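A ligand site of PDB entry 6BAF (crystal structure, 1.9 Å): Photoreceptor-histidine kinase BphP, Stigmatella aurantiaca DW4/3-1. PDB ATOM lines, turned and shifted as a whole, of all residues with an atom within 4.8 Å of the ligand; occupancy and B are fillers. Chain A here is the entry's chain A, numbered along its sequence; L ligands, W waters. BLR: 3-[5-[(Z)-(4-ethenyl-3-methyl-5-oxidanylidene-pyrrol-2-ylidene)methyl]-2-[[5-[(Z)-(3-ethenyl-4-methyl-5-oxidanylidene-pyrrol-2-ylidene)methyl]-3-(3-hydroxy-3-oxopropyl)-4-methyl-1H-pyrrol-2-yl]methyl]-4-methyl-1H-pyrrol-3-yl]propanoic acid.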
ATOM      1  N   CYS A   3      -4.884 -37.011  34.832  1.00  0.00           N
ATOM      2  CA  CYS A   3      -4.680 -35.569  34.673  1.00  0.00           C
ATOM      3  C   CYS A   3      -5.279 -34.762  35.819  1.00  0.00           C
ATOM      4  O   CYS A   3      -4.713 -33.723  36.212  1.00  0.00           O
ATOM      5  CB  CYS A   3      -5.302 -35.119  33.346  1.00  0.00           C
ATOM      6  SG  CYS A   3      -4.466 -35.926  31.953  1.00  0.00           S
ATOM      7  N   GLU A   6      -3.054 -33.814  39.890  1.00  0.00           N
ATOM      8  CA  GLU A   6      -2.032 -32.855  40.271  1.00  0.00           C
ATOM      9  C   GLU A   6      -2.698 -31.617  40.884  1.00  0.00           C
ATOM     10  O   GLU A   6      -3.673 -31.118  40.319  1.00  0.00           O
ATOM     11  CB  GLU A   6      -1.218 -32.432  39.050  1.00  0.00           C
ATOM     12  CG  GLU A   6      -0.349 -31.226  39.312  1.00  0.00           C
ATOM     13  CD  GLU A   6       0.040 -30.482  38.021  1.00  0.00           C
ATOM     14  OE1 GLU A   6      -0.597 -30.804  36.953  1.00  0.00           O
ATOM     15  OE2 GLU A   6       0.954 -29.608  38.103  1.00  0.00           O
ATOM     16  N   ILE A   8      -2.098 -27.950  41.684  1.00  0.00           N
ATOM     17  CA  ILE A   8      -1.946 -26.766  40.810  1.00  0.00           C
ATOM     18  C   ILE A   8      -2.126 -25.493  41.608  1.00  0.00           C
ATOM     19  O   ILE A   8      -1.449 -24.500  41.312  1.00  0.00           O
ATOM     20  CB  ILE A   8      -2.805 -26.736  39.503  1.00  0.00           C
ATOM     21  CG1 ILE A   8      -4.245 -26.208  39.679  1.00  0.00           C
ATOM     22  CG2 ILE A   8      -2.614 -28.046  38.640  1.00  0.00           C
ATOM     23  CD1 ILE A   8      -4.925 -25.894  38.350  1.00  0.00           C
ATOM     24  N   ILE A 160      -9.110 -17.359  20.619  1.00  0.00           N
ATOM     25  CA  ILE A 160     -10.214 -18.236  20.273  1.00  0.00           C
ATOM     26  C   ILE A 160     -11.262 -18.172  21.360  1.00  0.00           C
ATOM     27  O   ILE A 160     -10.983 -17.776  22.497  1.00  0.00           O
ATOM     28  CB  ILE A 160      -9.744 -19.694  20.048  1.00  0.00           C
ATOM     29  CG1 ILE A 160      -9.177 -20.293  21.355  1.00  0.00           C
ATOM     30  CG2 ILE A 160      -8.685 -19.728  18.934  1.00  0.00           C
ATOM     31  CD1 ILE A 160      -9.099 -21.868  21.372  1.00  0.00           C
ATOM     32  N   TYR A 162     -13.188 -21.085  23.195  1.00  0.00           N
ATOM     33  CA  TYR A 162     -13.069 -22.520  23.395  1.00  0.00           C
ATOM     34  C   TYR A 162     -14.276 -22.920  24.227  1.00  0.00           C
ATOM     35  O   TYR A 162     -14.390 -22.548  25.384  1.00  0.00           O
ATOM     36  CB  TYR A 162     -11.767 -22.823  24.110  1.00  0.00           C
ATOM     37  CG  TYR A 162     -11.443 -24.306  24.264  1.00  0.00           C
ATOM     38  CD1 TYR A 162     -10.937 -25.044  23.185  1.00  0.00           C
ATOM     39  CD2 TYR A 162     -11.638 -24.969  25.486  1.00  0.00           C
ATOM     40  CE1 TYR A 162     -10.626 -26.412  23.319  1.00  0.00           C
ATOM     41  CE2 TYR A 162     -11.327 -26.341  25.633  1.00  0.00           C
ATOM     42  CZ  TYR A 162     -10.821 -27.045  24.544  1.00  0.00           C
ATOM     43  OH  TYR A 162     -10.500 -28.384  24.650  1.00  0.00           O
ATOM     44  N   VAL A 172     -13.069 -25.364  19.329  1.00  0.00           N
ATOM     45  CA  VAL A 172     -12.684 -24.021  18.898  1.00  0.00           C
ATOM     46  C   VAL A 172     -13.798 -23.508  17.986  1.00  0.00           C
ATOM     47  O   VAL A 172     -13.848 -23.836  16.792  1.00  0.00           O
ATOM     48  CB  VAL A 172     -11.336 -24.011  18.188  1.00  0.00           C
ATOM     49  CG1 VAL A 172     -10.982 -22.571  17.804  1.00  0.00           C
ATOM     50  CG2 VAL A 172     -10.272 -24.649  19.087  1.00  0.00           C
ATOM     51  N   TYR A 184      -6.782 -23.038  14.281  1.00  0.00           N
ATOM     52  CA  TYR A 184      -7.364 -24.108  15.074  1.00  0.00           C
ATOM     53  C   TYR A 184      -8.881 -24.129  14.973  1.00  0.00           C
ATOM     54  O   TYR A 184      -9.524 -24.979  15.601  1.00  0.00           O
ATOM     55  CB  TYR A 184      -6.947 -23.979  16.530  1.00  0.00           C
ATOM     56  CG  TYR A 184      -5.471 -24.142  16.762  1.00  0.00           C
ATOM     57  CD1 TYR A 184      -4.650 -24.798  15.840  1.00  0.00           C
ATOM     58  CD2 TYR A 184      -4.890 -23.660  17.914  1.00  0.00           C
ATOM     59  CE1 TYR A 184      -3.290 -24.958  16.087  1.00  0.00           C
ATOM     60  CE2 TYR A 184      -3.536 -23.813  18.156  1.00  0.00           C
ATOM     61  CZ  TYR A 184      -2.743 -24.469  17.241  1.00  0.00           C
ATOM     62  OH  TYR A 184      -1.391 -24.610  17.503  1.00  0.00           O
ATOM     63  N   PHE A 189     -11.141 -31.098  21.119  1.00  0.00           N
ATOM     64  CA  PHE A 189     -10.047 -31.614  21.925  1.00  0.00           C
ATOM     65  C   PHE A 189     -10.636 -32.374  23.107  1.00  0.00           C
ATOM     66  O   PHE A 189     -11.763 -32.098  23.519  1.00  0.00           O
ATOM     67  CB  PHE A 189      -9.118 -30.499  22.478  1.00  0.00           C
ATOM     68  CG  PHE A 189      -8.347 -29.751  21.405  1.00  0.00           C
ATOM     69  CD1 PHE A 189      -8.956 -28.750  20.654  1.00  0.00           C
ATOM     70  CD2 PHE A 189      -7.006 -30.027  21.188  1.00  0.00           C
ATOM     71  CE1 PHE A 189      -8.248 -28.062  19.694  1.00  0.00           C
ATOM     72  CE2 PHE A 189      -6.289 -29.349  20.226  1.00  0.00           C
ATOM     73  CZ  PHE A 189      -6.924 -28.330  19.465  1.00  0.00           C
ATOM     74  N   SER A 192      -9.343 -33.990  28.864  1.00  0.00           N
ATOM     75  CA  SER A 192      -8.175 -33.961  29.743  1.00  0.00           C
ATOM     76  C   SER A 192      -7.205 -32.849  29.399  1.00  0.00           C
ATOM     77  O   SER A 192      -6.314 -32.560  30.217  1.00  0.00           O
ATOM     78  CB  SER A 192      -7.435 -35.316  29.725  1.00  0.00           C
ATOM     79  OG  SER A 192      -7.493 -35.912  28.432  1.00  0.00           O
ATOM     80  N   ASP A 193      -7.343 -32.188  28.249  1.00  0.00           N
ATOM     81  CA  ASP A 193      -6.412 -31.106  27.940  1.00  0.00           C
ATOM     82  C   ASP A 193      -6.596 -29.923  28.872  1.00  0.00           C
ATOM     83  O   ASP A 193      -5.656 -29.134  29.068  1.00  0.00           O
ATOM     84  CB  ASP A 193      -6.574 -30.647  26.505  1.00  0.00           C
ATOM     85  CG  ASP A 193      -6.042 -31.661  25.505  1.00  0.00           C
ATOM     86  OD1 ASP A 193      -5.639 -32.780  25.924  1.00  0.00           O
ATOM     87  OD2 ASP A 193      -6.008 -31.336  24.308  1.00  0.00           O
ATOM     88  N   ILE A 194      -7.772 -29.781  29.478  1.00  0.00           N
ATOM     89  CA  ILE A 194      -7.948 -28.811  30.553  1.00  0.00           C
ATOM     90  C   ILE A 194      -8.579 -29.612  31.676  1.00  0.00           C
ATOM     91  O   ILE A 194      -9.812 -29.702  31.784  1.00  0.00           O
ATOM     92  CB  ILE A 194      -8.814 -27.613  30.130  1.00  0.00           C
ATOM     93  CG1 ILE A 194      -8.344 -27.060  28.765  1.00  0.00           C
ATOM     94  CG2 ILE A 194      -8.804 -26.534  31.266  1.00  0.00           C
ATOM     95  CD1 ILE A 194      -9.033 -25.714  28.325  1.00  0.00           C
ATOM     96  N   PRO A 195      -7.764 -30.217  32.541  1.00  0.00           N
ATOM     97  CA  PRO A 195      -8.281 -31.256  33.433  1.00  0.00           C
ATOM     98  C   PRO A 195      -9.126 -30.649  34.526  1.00  0.00           C
ATOM     99  O   PRO A 195      -9.202 -29.432  34.731  1.00  0.00           O
ATOM    100  CB  PRO A 195      -7.017 -31.929  33.992  1.00  0.00           C
ATOM    101  CG  PRO A 195      -5.951 -30.827  33.899  1.00  0.00           C
ATOM    102  CD  PRO A 195      -6.307 -30.047  32.632  1.00  0.00           C
ATOM    103  N   GLN A 197      -9.345 -30.375  37.867  1.00  0.00           N
ATOM    104  CA  GLN A 197      -9.004 -29.404  38.893  1.00  0.00           C
ATOM    105  C   GLN A 197      -8.648 -28.031  38.293  1.00  0.00           C
ATOM    106  O   GLN A 197      -8.763 -27.019  38.995  1.00  0.00           O
ATOM    107  CB  GLN A 197      -7.845 -29.940  39.767  1.00  0.00           C
ATOM    108  CG  GLN A 197      -6.435 -29.807  39.174  1.00  0.00           C
ATOM    109  CD  GLN A 197      -6.107 -30.842  38.098  1.00  0.00           C
ATOM    110  OE1 GLN A 197      -6.978 -31.235  37.290  1.00  0.00           O
ATOM    111  NE2 GLN A 197      -4.853 -31.288  38.077  1.00  0.00           N
ATOM    112  N   ALA A 198      -8.212 -27.972  37.029  1.00  0.00           N
ATOM    113  CA  ALA A 198      -8.027 -26.672  36.389  1.00  0.00           C
ATOM    114  C   ALA A 198      -9.379 -26.027  36.112  1.00  0.00           C
ATOM    115  O   ALA A 198      -9.597 -24.850  36.452  1.00  0.00           O
ATOM    116  CB  ALA A 198      -7.234 -26.820  35.086  1.00  0.00           C
ATOM    117  N   TYR A 202     -10.821 -22.561  37.451  1.00  0.00           N
ATOM    118  CA  TYR A 202     -11.152 -21.477  36.533  1.00  0.00           C
ATOM    119  C   TYR A 202     -12.593 -21.039  36.701  1.00  0.00           C
ATOM    120  O   TYR A 202     -12.961 -19.958  36.231  1.00  0.00           O
ATOM    121  CB  TYR A 202     -10.884 -21.861  35.074  1.00  0.00           C
ATOM    122  CG  TYR A 202      -9.438 -22.266  34.791  1.00  0.00           C
ATOM    123  CD1 TYR A 202      -8.402 -21.931  35.677  1.00  0.00           C
ATOM    124  CD2 TYR A 202      -9.114 -22.971  33.633  1.00  0.00           C
ATOM    125  CE1 TYR A 202      -7.087 -22.320  35.421  1.00  0.00           C
ATOM    126  CE2 TYR A 202      -7.786 -23.348  33.345  1.00  0.00           C
ATOM    127  CZ  TYR A 202      -6.790 -23.038  34.252  1.00  0.00           C
ATOM    128  OH  TYR A 202      -5.487 -23.388  33.965  1.00  0.00           O
ATOM    129  N   ARG A 208      -6.172 -15.873  33.739  1.00  0.00           N
ATOM    130  CA  ARG A 208      -4.829 -16.370  33.977  1.00  0.00           C
ATOM    131  C   ARG A 208      -3.961 -15.882  32.838  1.00  0.00           C
ATOM    132  O   ARG A 208      -4.410 -15.801  31.692  1.00  0.00           O
ATOM    133  CB  ARG A 208      -4.779 -17.909  34.074  1.00  0.00           C
ATOM    134  CG  ARG A 208      -5.343 -18.607  32.857  1.00  0.00           C
ATOM    135  CD  ARG A 208      -6.324 -19.686  33.279  1.00  0.00           C
ATOM    136  NE  ARG A 208      -7.485 -19.197  34.047  1.00  0.00           N
ATOM    137  CZ  ARG A 208      -8.684 -18.995  33.508  1.00  0.00           C
ATOM    138  NH1 ARG A 208      -9.705 -18.566  34.256  1.00  0.00           N
ATOM    139  NH2 ARG A 208      -8.862 -19.213  32.193  1.00  0.00           N
ATOM    140  N   ILE A 210       0.189 -16.222  31.292  1.00  0.00           N
ATOM    141  CA  ILE A 210       1.556 -16.749  31.266  1.00  0.00           C
ATOM    142  C   ILE A 210       2.318 -15.941  30.228  1.00  0.00           C
ATOM    143  O   ILE A 210       2.284 -16.276  29.046  1.00  0.00           O
ATOM    144  CB  ILE A 210       1.538 -18.244  30.915  1.00  0.00           C
ATOM    145  CG1 ILE A 210       0.563 -18.981  31.819  1.00  0.00           C
ATOM    146  CG2 ILE A 210       2.974 -18.854  30.943  1.00  0.00           C
ATOM    147  CD1 ILE A 210       0.162 -20.352  31.292  1.00  0.00           C
ATOM    148  N   ARG A 238       0.715 -16.949  40.240  1.00  0.00           N
ATOM    149  CA  ARG A 238       0.841 -18.380  40.539  1.00  0.00           C
ATOM    150  C   ARG A 238       1.599 -19.114  39.425  1.00  0.00           C
ATOM    151  O   ARG A 238       1.233 -19.025  38.252  1.00  0.00           O
ATOM    152  CB  ARG A 238      -0.550 -19.009  40.702  1.00  0.00           C
ATOM    153  CG  ARG A 238      -0.556 -20.530  40.976  1.00  0.00           C
ATOM    154  CD  ARG A 238      -1.986 -21.113  41.043  1.00  0.00           C
ATOM    155  NE  ARG A 238      -2.710 -20.899  39.792  1.00  0.00           N
ATOM    156  CZ  ARG A 238      -2.664 -21.733  38.754  1.00  0.00           C
ATOM    157  NH1 ARG A 238      -3.319 -21.429  37.646  1.00  0.00           N
ATOM    158  NH2 ARG A 238      -1.950 -22.872  38.832  1.00  0.00           N
ATOM    159  N   SER A 239       2.642 -19.858  39.794  1.00  0.00           N
ATOM    160  CA  SER A 239       3.356 -20.651  38.817  1.00  0.00           C
ATOM    161  C   SER A 239       2.461 -21.752  38.291  1.00  0.00           C
ATOM    162  O   SER A 239       1.814 -22.466  39.077  1.00  0.00           O
ATOM    163  CB  SER A 239       4.628 -21.246  39.440  1.00  0.00           C
ATOM    164  OG  SER A 239       5.399 -21.859  38.427  1.00  0.00           O
ATOM    165  N   VAL A 240       2.409 -21.928  36.976  1.00  0.00           N
ATOM    166  CA  VAL A 240       1.366 -22.845  36.498  1.00  0.00           C
ATOM    167  C   VAL A 240       1.928 -24.250  36.357  1.00  0.00           C
ATOM    168  O   VAL A 240       3.139 -24.464  36.393  1.00  0.00           O
ATOM    169  CB  VAL A 240       0.724 -22.374  35.177  1.00  0.00           C
ATOM    170  CG1 VAL A 240       0.128 -20.936  35.336  1.00  0.00           C
ATOM    171  CG2 VAL A 240       1.719 -22.487  34.051  1.00  0.00           C
ATOM    172  N   SER A 241       1.033 -25.206  36.180  1.00  0.00           N
ATOM    173  CA  SER A 241       1.455 -26.597  36.193  1.00  0.00           C
ATOM    174  C   SER A 241       2.535 -26.870  35.155  1.00  0.00           C
ATOM    175  O   SER A 241       2.386 -26.468  33.984  1.00  0.00           O
ATOM    176  CB  SER A 241       0.252 -27.486  35.985  1.00  0.00           C
ATOM    177  OG  SER A 241       0.622 -28.696  35.373  1.00  0.00           O
ATOM    178  N   ILE A 243       3.321 -29.495  33.555  1.00  0.00           N
ATOM    179  CA  ILE A 243       2.912 -30.263  32.389  1.00  0.00           C
ATOM    180  C   ILE A 243       2.173 -29.385  31.386  1.00  0.00           C
ATOM    181  O   ILE A 243       2.172 -29.672  30.183  1.00  0.00           O
ATOM    182  CB  ILE A 243       2.068 -31.463  32.845  1.00  0.00           C
ATOM    183  CG1 ILE A 243       1.698 -32.351  31.669  1.00  0.00           C
ATOM    184  CG2 ILE A 243       0.792 -31.027  33.468  1.00  0.00           C
ATOM    185  CD1 ILE A 243       1.062 -33.680  32.082  1.00  0.00           C
ATOM    186  N   HIS A 244       1.479 -28.328  31.848  1.00  0.00           N
ATOM    187  CA  HIS A 244       0.867 -27.422  30.885  1.00  0.00           C
ATOM    188  C   HIS A 244       1.929 -26.623  30.144  1.00  0.00           C
ATOM    189  O   HIS A 244       1.812 -26.403  28.941  1.00  0.00           O
ATOM    190  CB  HIS A 244      -0.137 -26.479  31.576  1.00  0.00           C
ATOM    191  CG  HIS A 244      -0.807 -25.539  30.617  1.00  0.00           C
ATOM    192  ND1 HIS A 244      -1.501 -25.984  29.508  1.00  0.00           N
ATOM    193  CD2 HIS A 244      -0.844 -24.189  30.575  1.00  0.00           C
ATOM    194  CE1 HIS A 244      -1.962 -24.949  28.843  1.00  0.00           C
ATOM    195  NE2 HIS A 244      -1.591 -23.845  29.473  1.00  0.00           N
ATOM    196  N   TYR A 247       2.935 -28.830  27.365  1.00  0.00           N
ATOM    197  CA  TYR A 247       1.935 -28.733  26.327  1.00  0.00           C
ATOM    198  C   TYR A 247       2.146 -27.492  25.457  1.00  0.00           C
ATOM    199  O   TYR A 247       2.050 -27.568  24.229  1.00  0.00           O
ATOM    200  CB  TYR A 247       0.554 -28.678  26.962  1.00  0.00           C
ATOM    201  CG  TYR A 247      -0.630 -28.647  26.006  1.00  0.00           C
ATOM    202  CD1 TYR A 247      -1.191 -29.830  25.602  1.00  0.00           C
ATOM    203  CD2 TYR A 247      -1.254 -27.448  25.590  1.00  0.00           C
ATOM    204  CE1 TYR A 247      -2.279 -29.875  24.822  1.00  0.00           C
ATOM    205  CE2 TYR A 247      -2.424 -27.491  24.714  1.00  0.00           C
ATOM    206  CZ  TYR A 247      -2.910 -28.724  24.345  1.00  0.00           C
ATOM    207  OH  TYR A 247      -4.029 -28.940  23.530  1.00  0.00           O
ATOM    208  N   LEU A 248       2.416 -26.328  26.070  1.00  0.00           N
ATOM    209  CA  LEU A 248       2.533 -25.093  25.303  1.00  0.00           C
ATOM    210  C   LEU A 248       3.781 -25.148  24.436  1.00  0.00           C
ATOM    211  O   LEU A 248       3.720 -24.852  23.230  1.00  0.00           O
ATOM    212  CB  LEU A 248       2.559 -23.868  26.235  1.00  0.00           C
ATOM    213  CG  LEU A 248       1.216 -23.551  26.929  1.00  0.00           C
ATOM    214  CD1 LEU A 248       1.194 -22.289  27.821  1.00  0.00           C
ATOM    215  CD2 LEU A 248       0.137 -23.509  25.910  1.00  0.00           C
ATOM    216  N   MET A 251       3.132 -27.350  21.528  1.00  0.00           N
ATOM    217  CA  MET A 251       2.240 -26.728  20.601  1.00  0.00           C
ATOM    218  C   MET A 251       2.937 -25.595  19.831  1.00  0.00           C
ATOM    219  O   MET A 251       2.350 -25.065  18.882  1.00  0.00           O
ATOM    220  CB  MET A 251       1.030 -26.250  21.381  1.00  0.00           C
ATOM    221  CG  MET A 251      -0.185 -26.167  20.606  1.00  0.00           C
ATOM    222  SD  MET A 251      -1.415 -25.661  21.783  1.00  0.00           S
ATOM    223  CE  MET A 251      -1.975 -24.139  21.075  1.00  0.00           C
ATOM    224  N   SER A 256       0.658 -17.135  26.801  1.00  0.00           N
ATOM    225  CA  SER A 256      -0.750 -17.506  26.813  1.00  0.00           C
ATOM    226  C   SER A 256      -1.526 -16.598  27.754  1.00  0.00           C
ATOM    227  O   SER A 256      -0.972 -16.103  28.731  1.00  0.00           O
ATOM    228  CB  SER A 256      -0.928 -18.950  27.300  1.00  0.00           C
ATOM    229  OG  SER A 256      -2.220 -19.383  27.015  1.00  0.00           O
ATOM    230  N   MET A 257      -2.822 -16.444  27.497  1.00  0.00           N
ATOM    231  CA  MET A 257      -3.729 -15.811  28.449  1.00  0.00           C
ATOM    232  C   MET A 257      -5.108 -16.389  28.197  1.00  0.00           C
ATOM    233  O   MET A 257      -5.475 -16.569  27.037  1.00  0.00           O
ATOM    234  CB  MET A 257      -3.747 -14.265  28.273  1.00  0.00           C
ATOM    235  CG  MET A 257      -4.728 -13.526  29.208  1.00  0.00           C
ATOM    236  SD  MET A 257      -4.828 -11.687  28.952  1.00  0.00           S
ATOM    237  CE  MET A 257      -5.862 -11.651  27.483  1.00  0.00           C
ATOM    238  N   SER A 258      -5.851 -16.728  29.252  1.00  0.00           N
ATOM    239  CA  SER A 258      -7.226 -17.152  29.037  1.00  0.00           C
ATOM    240  C   SER A 258      -8.137 -16.514  30.081  1.00  0.00           C
ATOM    241  O   SER A 258      -7.693 -16.061  31.139  1.00  0.00           O
ATOM    242  CB  SER A 258      -7.397 -18.691  29.006  1.00  0.00           C
ATOM    243  OG  SER A 258      -6.825 -19.306  30.165  1.00  0.00           O
ATOM    244  N   LEU A 270     -13.833 -20.705  27.371  1.00  0.00           N
ATOM    245  CA  LEU A 270     -12.717 -19.835  27.655  1.00  0.00           C
ATOM    246  C   LEU A 270     -12.541 -18.926  26.463  1.00  0.00           C
ATOM    247  O   LEU A 270     -12.799 -19.334  25.331  1.00  0.00           O
ATOM    248  CB  LEU A 270     -11.386 -20.587  27.858  1.00  0.00           C
ATOM    249  CG  LEU A 270     -11.195 -21.660  28.943  1.00  0.00           C
ATOM    250  CD1 LEU A 270      -9.747 -22.111  28.831  1.00  0.00           C
ATOM    251  CD2 LEU A 270     -11.462 -21.091  30.308  1.00  0.00           C
ATOM    252  N   SER A 272      -9.303 -17.877  24.909  1.00  0.00           N
ATOM    253  CA  SER A 272      -7.936 -18.360  25.025  1.00  0.00           C
ATOM    254  C   SER A 272      -7.078 -17.638  24.010  1.00  0.00           C
ATOM    255  O   SER A 272      -7.387 -17.673  22.825  1.00  0.00           O
ATOM    256  CB  SER A 272      -7.862 -19.906  24.791  1.00  0.00           C
ATOM    257  OG  SER A 272      -6.492 -20.339  24.796  1.00  0.00           O
ATOM    258  N   THR A 274      -3.017 -16.979  22.527  1.00  0.00           N
ATOM    259  CA  THR A 274      -1.709 -17.613  22.465  1.00  0.00           C
ATOM    260  C   THR A 274      -0.808 -16.804  21.554  1.00  0.00           C
ATOM    261  O   THR A 274      -1.264 -16.170  20.589  1.00  0.00           O
ATOM    262  CB  THR A 274      -1.809 -19.086  21.964  1.00  0.00           C
ATOM    263  OG1 THR A 274      -2.662 -19.135  20.817  1.00  0.00           O
ATOM    264  CG2 THR A 274      -2.454 -19.997  23.042  1.00  0.00           C
HETATM  265  CHA BLR L   1      -4.484 -25.594  31.507  1.00  0.00           C
HETATM  266  NA  BLR L   1      -4.887 -26.150  29.069  1.00  0.00           N
HETATM  267  C1A BLR L   1      -4.904 -25.281  30.089  1.00  0.00           C
HETATM  268  C2A BLR L   1      -5.364 -24.033  29.668  1.00  0.00           C
HETATM  269  C3A BLR L   1      -5.665 -24.130  28.364  1.00  0.00           C
HETATM  270  C4A BLR L   1      -5.354 -25.449  27.992  1.00  0.00           C
HETATM  271  CMA BLR L   1      -6.253 -22.988  27.496  1.00  0.00           C
HETATM  272  CAA BLR L   1      -5.510 -22.804  30.571  1.00  0.00           C
HETATM  273  CBA BLR L   1      -4.173 -22.037  30.775  1.00  0.00           C
HETATM  274  CGA BLR L   1      -3.816 -21.184  29.550  1.00  0.00           C
HETATM  275  O1A BLR L   1      -4.641 -20.282  29.220  1.00  0.00           O
HETATM  276  O2A BLR L   1      -2.732 -21.352  28.876  1.00  0.00           O
HETATM  277  CHB BLR L   1      -5.496 -26.154  26.661  1.00  0.00           C
HETATM  278  NB  BLR L   1      -4.721 -24.351  25.088  1.00  0.00           N
HETATM  279  C1B BLR L   1      -5.467 -25.597  25.484  1.00  0.00           C
HETATM  280  C2B BLR L   1      -6.145 -26.098  24.258  1.00  0.00           C
HETATM  281  C3B BLR L   1      -5.887 -25.252  23.158  1.00  0.00           C
HETATM  282  C4B BLR L   1      -4.999 -24.130  23.601  1.00  0.00           C
HETATM  283  CMB BLR L   1      -7.034 -27.339  24.163  1.00  0.00           C
HETATM  284  OB  BLR L   1      -4.569 -23.246  22.947  1.00  0.00           O
HETATM  285  CAB BLR L   1      -6.483 -25.496  21.766  1.00  0.00           C
HETATM  286  CBB BLR L   1      -6.348 -24.630  20.792  1.00  0.00           C
HETATM  287  NC  BLR L   1      -2.917 -30.537  29.607  1.00  0.00           N
HETATM  288  C1C BLR L   1      -2.772 -31.697  28.645  1.00  0.00           C
HETATM  289  C2C BLR L   1      -2.542 -32.907  29.497  1.00  0.00           C
HETATM  290  C3C BLR L   1      -2.561 -32.579  30.878  1.00  0.00           C
HETATM  291  C4C BLR L   1      -2.786 -31.106  31.012  1.00  0.00           C
HETATM  292  CMC BLR L   1      -2.351 -34.278  28.904  1.00  0.00           C
HETATM  293  OC  BLR L   1      -2.807 -31.657  27.464  1.00  0.00           O
HETATM  294  CAC BLR L   1      -2.372 -33.570  32.043  1.00  0.00           C
HETATM  295  CBC BLR L   1      -3.104 -34.687  32.154  1.00  0.00           C
HETATM  296  CHD BLR L   1      -2.858 -30.456  32.129  1.00  0.00           C
HETATM  297  ND  BLR L   1      -3.787 -28.078  31.247  1.00  0.00           N
HETATM  298  C1D BLR L   1      -3.265 -29.008  32.262  1.00  0.00           C
HETATM  299  C2D BLR L   1      -3.136 -28.352  33.553  1.00  0.00           C
HETATM  300  C3D BLR L   1      -3.626 -26.982  33.375  1.00  0.00           C
HETATM  301  C4D BLR L   1      -4.057 -26.779  31.949  1.00  0.00           C
HETATM  302  CMD BLR L   1      -2.620 -28.996  34.844  1.00  0.00           C
HETATM  303  CAD BLR L   1      -3.670 -25.914  34.448  1.00  0.00           C
HETATM  304  CBD BLR L   1      -2.433 -25.033  34.295  1.00  0.00           C
HETATM  305  CGD BLR L   1      -2.561 -24.137  35.518  1.00  0.00           C
HETATM  306  O1D BLR L   1      -3.571 -23.360  35.622  1.00  0.00           O
HETATM  307  O2D BLR L   1      -1.703 -24.253  36.444  1.00  0.00           O
HETATM  308  O   HOH W   1      -1.700 -33.498  25.549  1.00  0.00           O
HETATM  309  O   HOH W   2      -2.576 -28.181  28.459  1.00  0.00           O
HETATM  310  O   HOH W   3      -3.109 -22.151  25.967  1.00  0.00           O
HETATM  311  O   HOH W   4      -4.745 -19.514  26.463  1.00  0.00           O
HETATM  312  O   HOH W   5      -6.027 -21.213  22.432  1.00  0.00           O
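Residues that only touch the ligand: Tyr 247 (3.1 Å), Pro 195 (3.2 Å), Val 240 (3.3 Å), Met 251 (3.3 Å), Tyr 184 (3.4 Å), Ile 243 (3.4 Å), Glu 6 (3.4 Å), Ile 194 (3.5 Å), Tyr 162 (3.7 Å), Phe 189 (3.7 Å), Ala 198 (3.7 Å), Ser 272 (3.8 Å), Ser 192 (3.8 Å), Leu 270 (3.8 Å), Thr 274 (3.9 Å), Ile 210 (3.9 Å), Ile 8 (3.9 Å) and Ile 160 (3.9 Å). Hydrophobic or aromatic side chains that line the ligand: Ile 8, Ile 160, Tyr 162, Tyr 184, Phe 189, Ile 194, Pro 195, Ala 198, Tyr 202, Ile 210, Val 240, Ile 243, His 244, Tyr 247, Met 251 and Leu 270. Of the 32 residues printed, 26 come within 4 Å of the ligand. Along chain A the residues within 4 Å of the ligand span positions 3 to 274. The nearest printed residue that does not touch the ligand is Met 257 (4.1 Å).
Water W5 lies within hydrogen-bond range of OB of the ligand (2.6 Å) and OG of Ser 272 (2.6 Å). Water W2 lies within hydrogen-bond range of a nitrogen (NC) of the ligand (2.6 Å), a ring nitrogen (ND1) of His 244 (2.7 Å) and the backbone carbonyl oxygen (O) of Asp 193 (3.3 Å). Water W4 lies within hydrogen-bond range of OG of Ser 272 (2.6 Å), OG of Ser 256 (2.6 Å), O1A of the ligand (2.9 Å) and O of Met 257 (3.1 Å). Water W3 bridges a nitrogen (NB) of the ligand and the side-chain hydroxyl (OG) of Ser 256.
OG of Ser 241 lies close to N of Ile 243 (3.4 Å). O of Ser 272 sits at hydrogen-bond distance from N of Ile 160, 2.8 Å away. The guanidinium group of Arg 238 sits at hydrogen-bond distance from the backbone carbonyl oxygen of Ile 8, 3.0 Å away. The backbone carbonyl oxygen (O) of Glu 6 is in hydrogen-bond range of the side-chain amide nitrogen (NE2) of Gln 197, 2.5 Å away. O of Ser 256 is in hydrogen-bond range of N of Ile 210, at 2.8 Å. The backbone carbonyl oxygen of Cys 3 is in hydrogen-bond range of the side-chain amide nitrogen of Gln 197 (3.1 Å). The side-chain hydroxyl (OG) of Ser 241 lies within hydrogen-bond range of the side-chain carboxylate (OE2) of Glu 6 (2.9 Å). OH of Tyr 247 sits at hydrogen-bond distance from OD2 of Asp 193.
ND of the ligand lies within hydrogen-bond range of O of Asp 193 (3.1 Å). The side-chain sulfur of Cys 3 is bonded to a carbon (CBC) of the ligand, at 1.9 Å. The side-chain hydroxyl (OH) of Tyr 202 is in hydrogen-bond range of an oxygen (O1D) of the ligand. The guanidinium group of Arg 238 lies within salt-bridge range of an oxygen (O2D) of the ligand (2.8 Å). The side-chain hydroxyl (OG) of Ser 256 sits at hydrogen-bond distance from an oxygen (O2A) of the ligand. A ring nitrogen (NE2) of His 244 is in hydrogen-bond range of an oxygen (O2A) of the ligand, 2.8 Å away. An oxygen (O2D) of the ligand lies within hydrogen-bond range of the backbone NH of Ser 241. The side-chain hydroxyl of Ser 258 sits at hydrogen-bond distance from an oxygen (O1A) of the ligand, 2.6 Å away.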
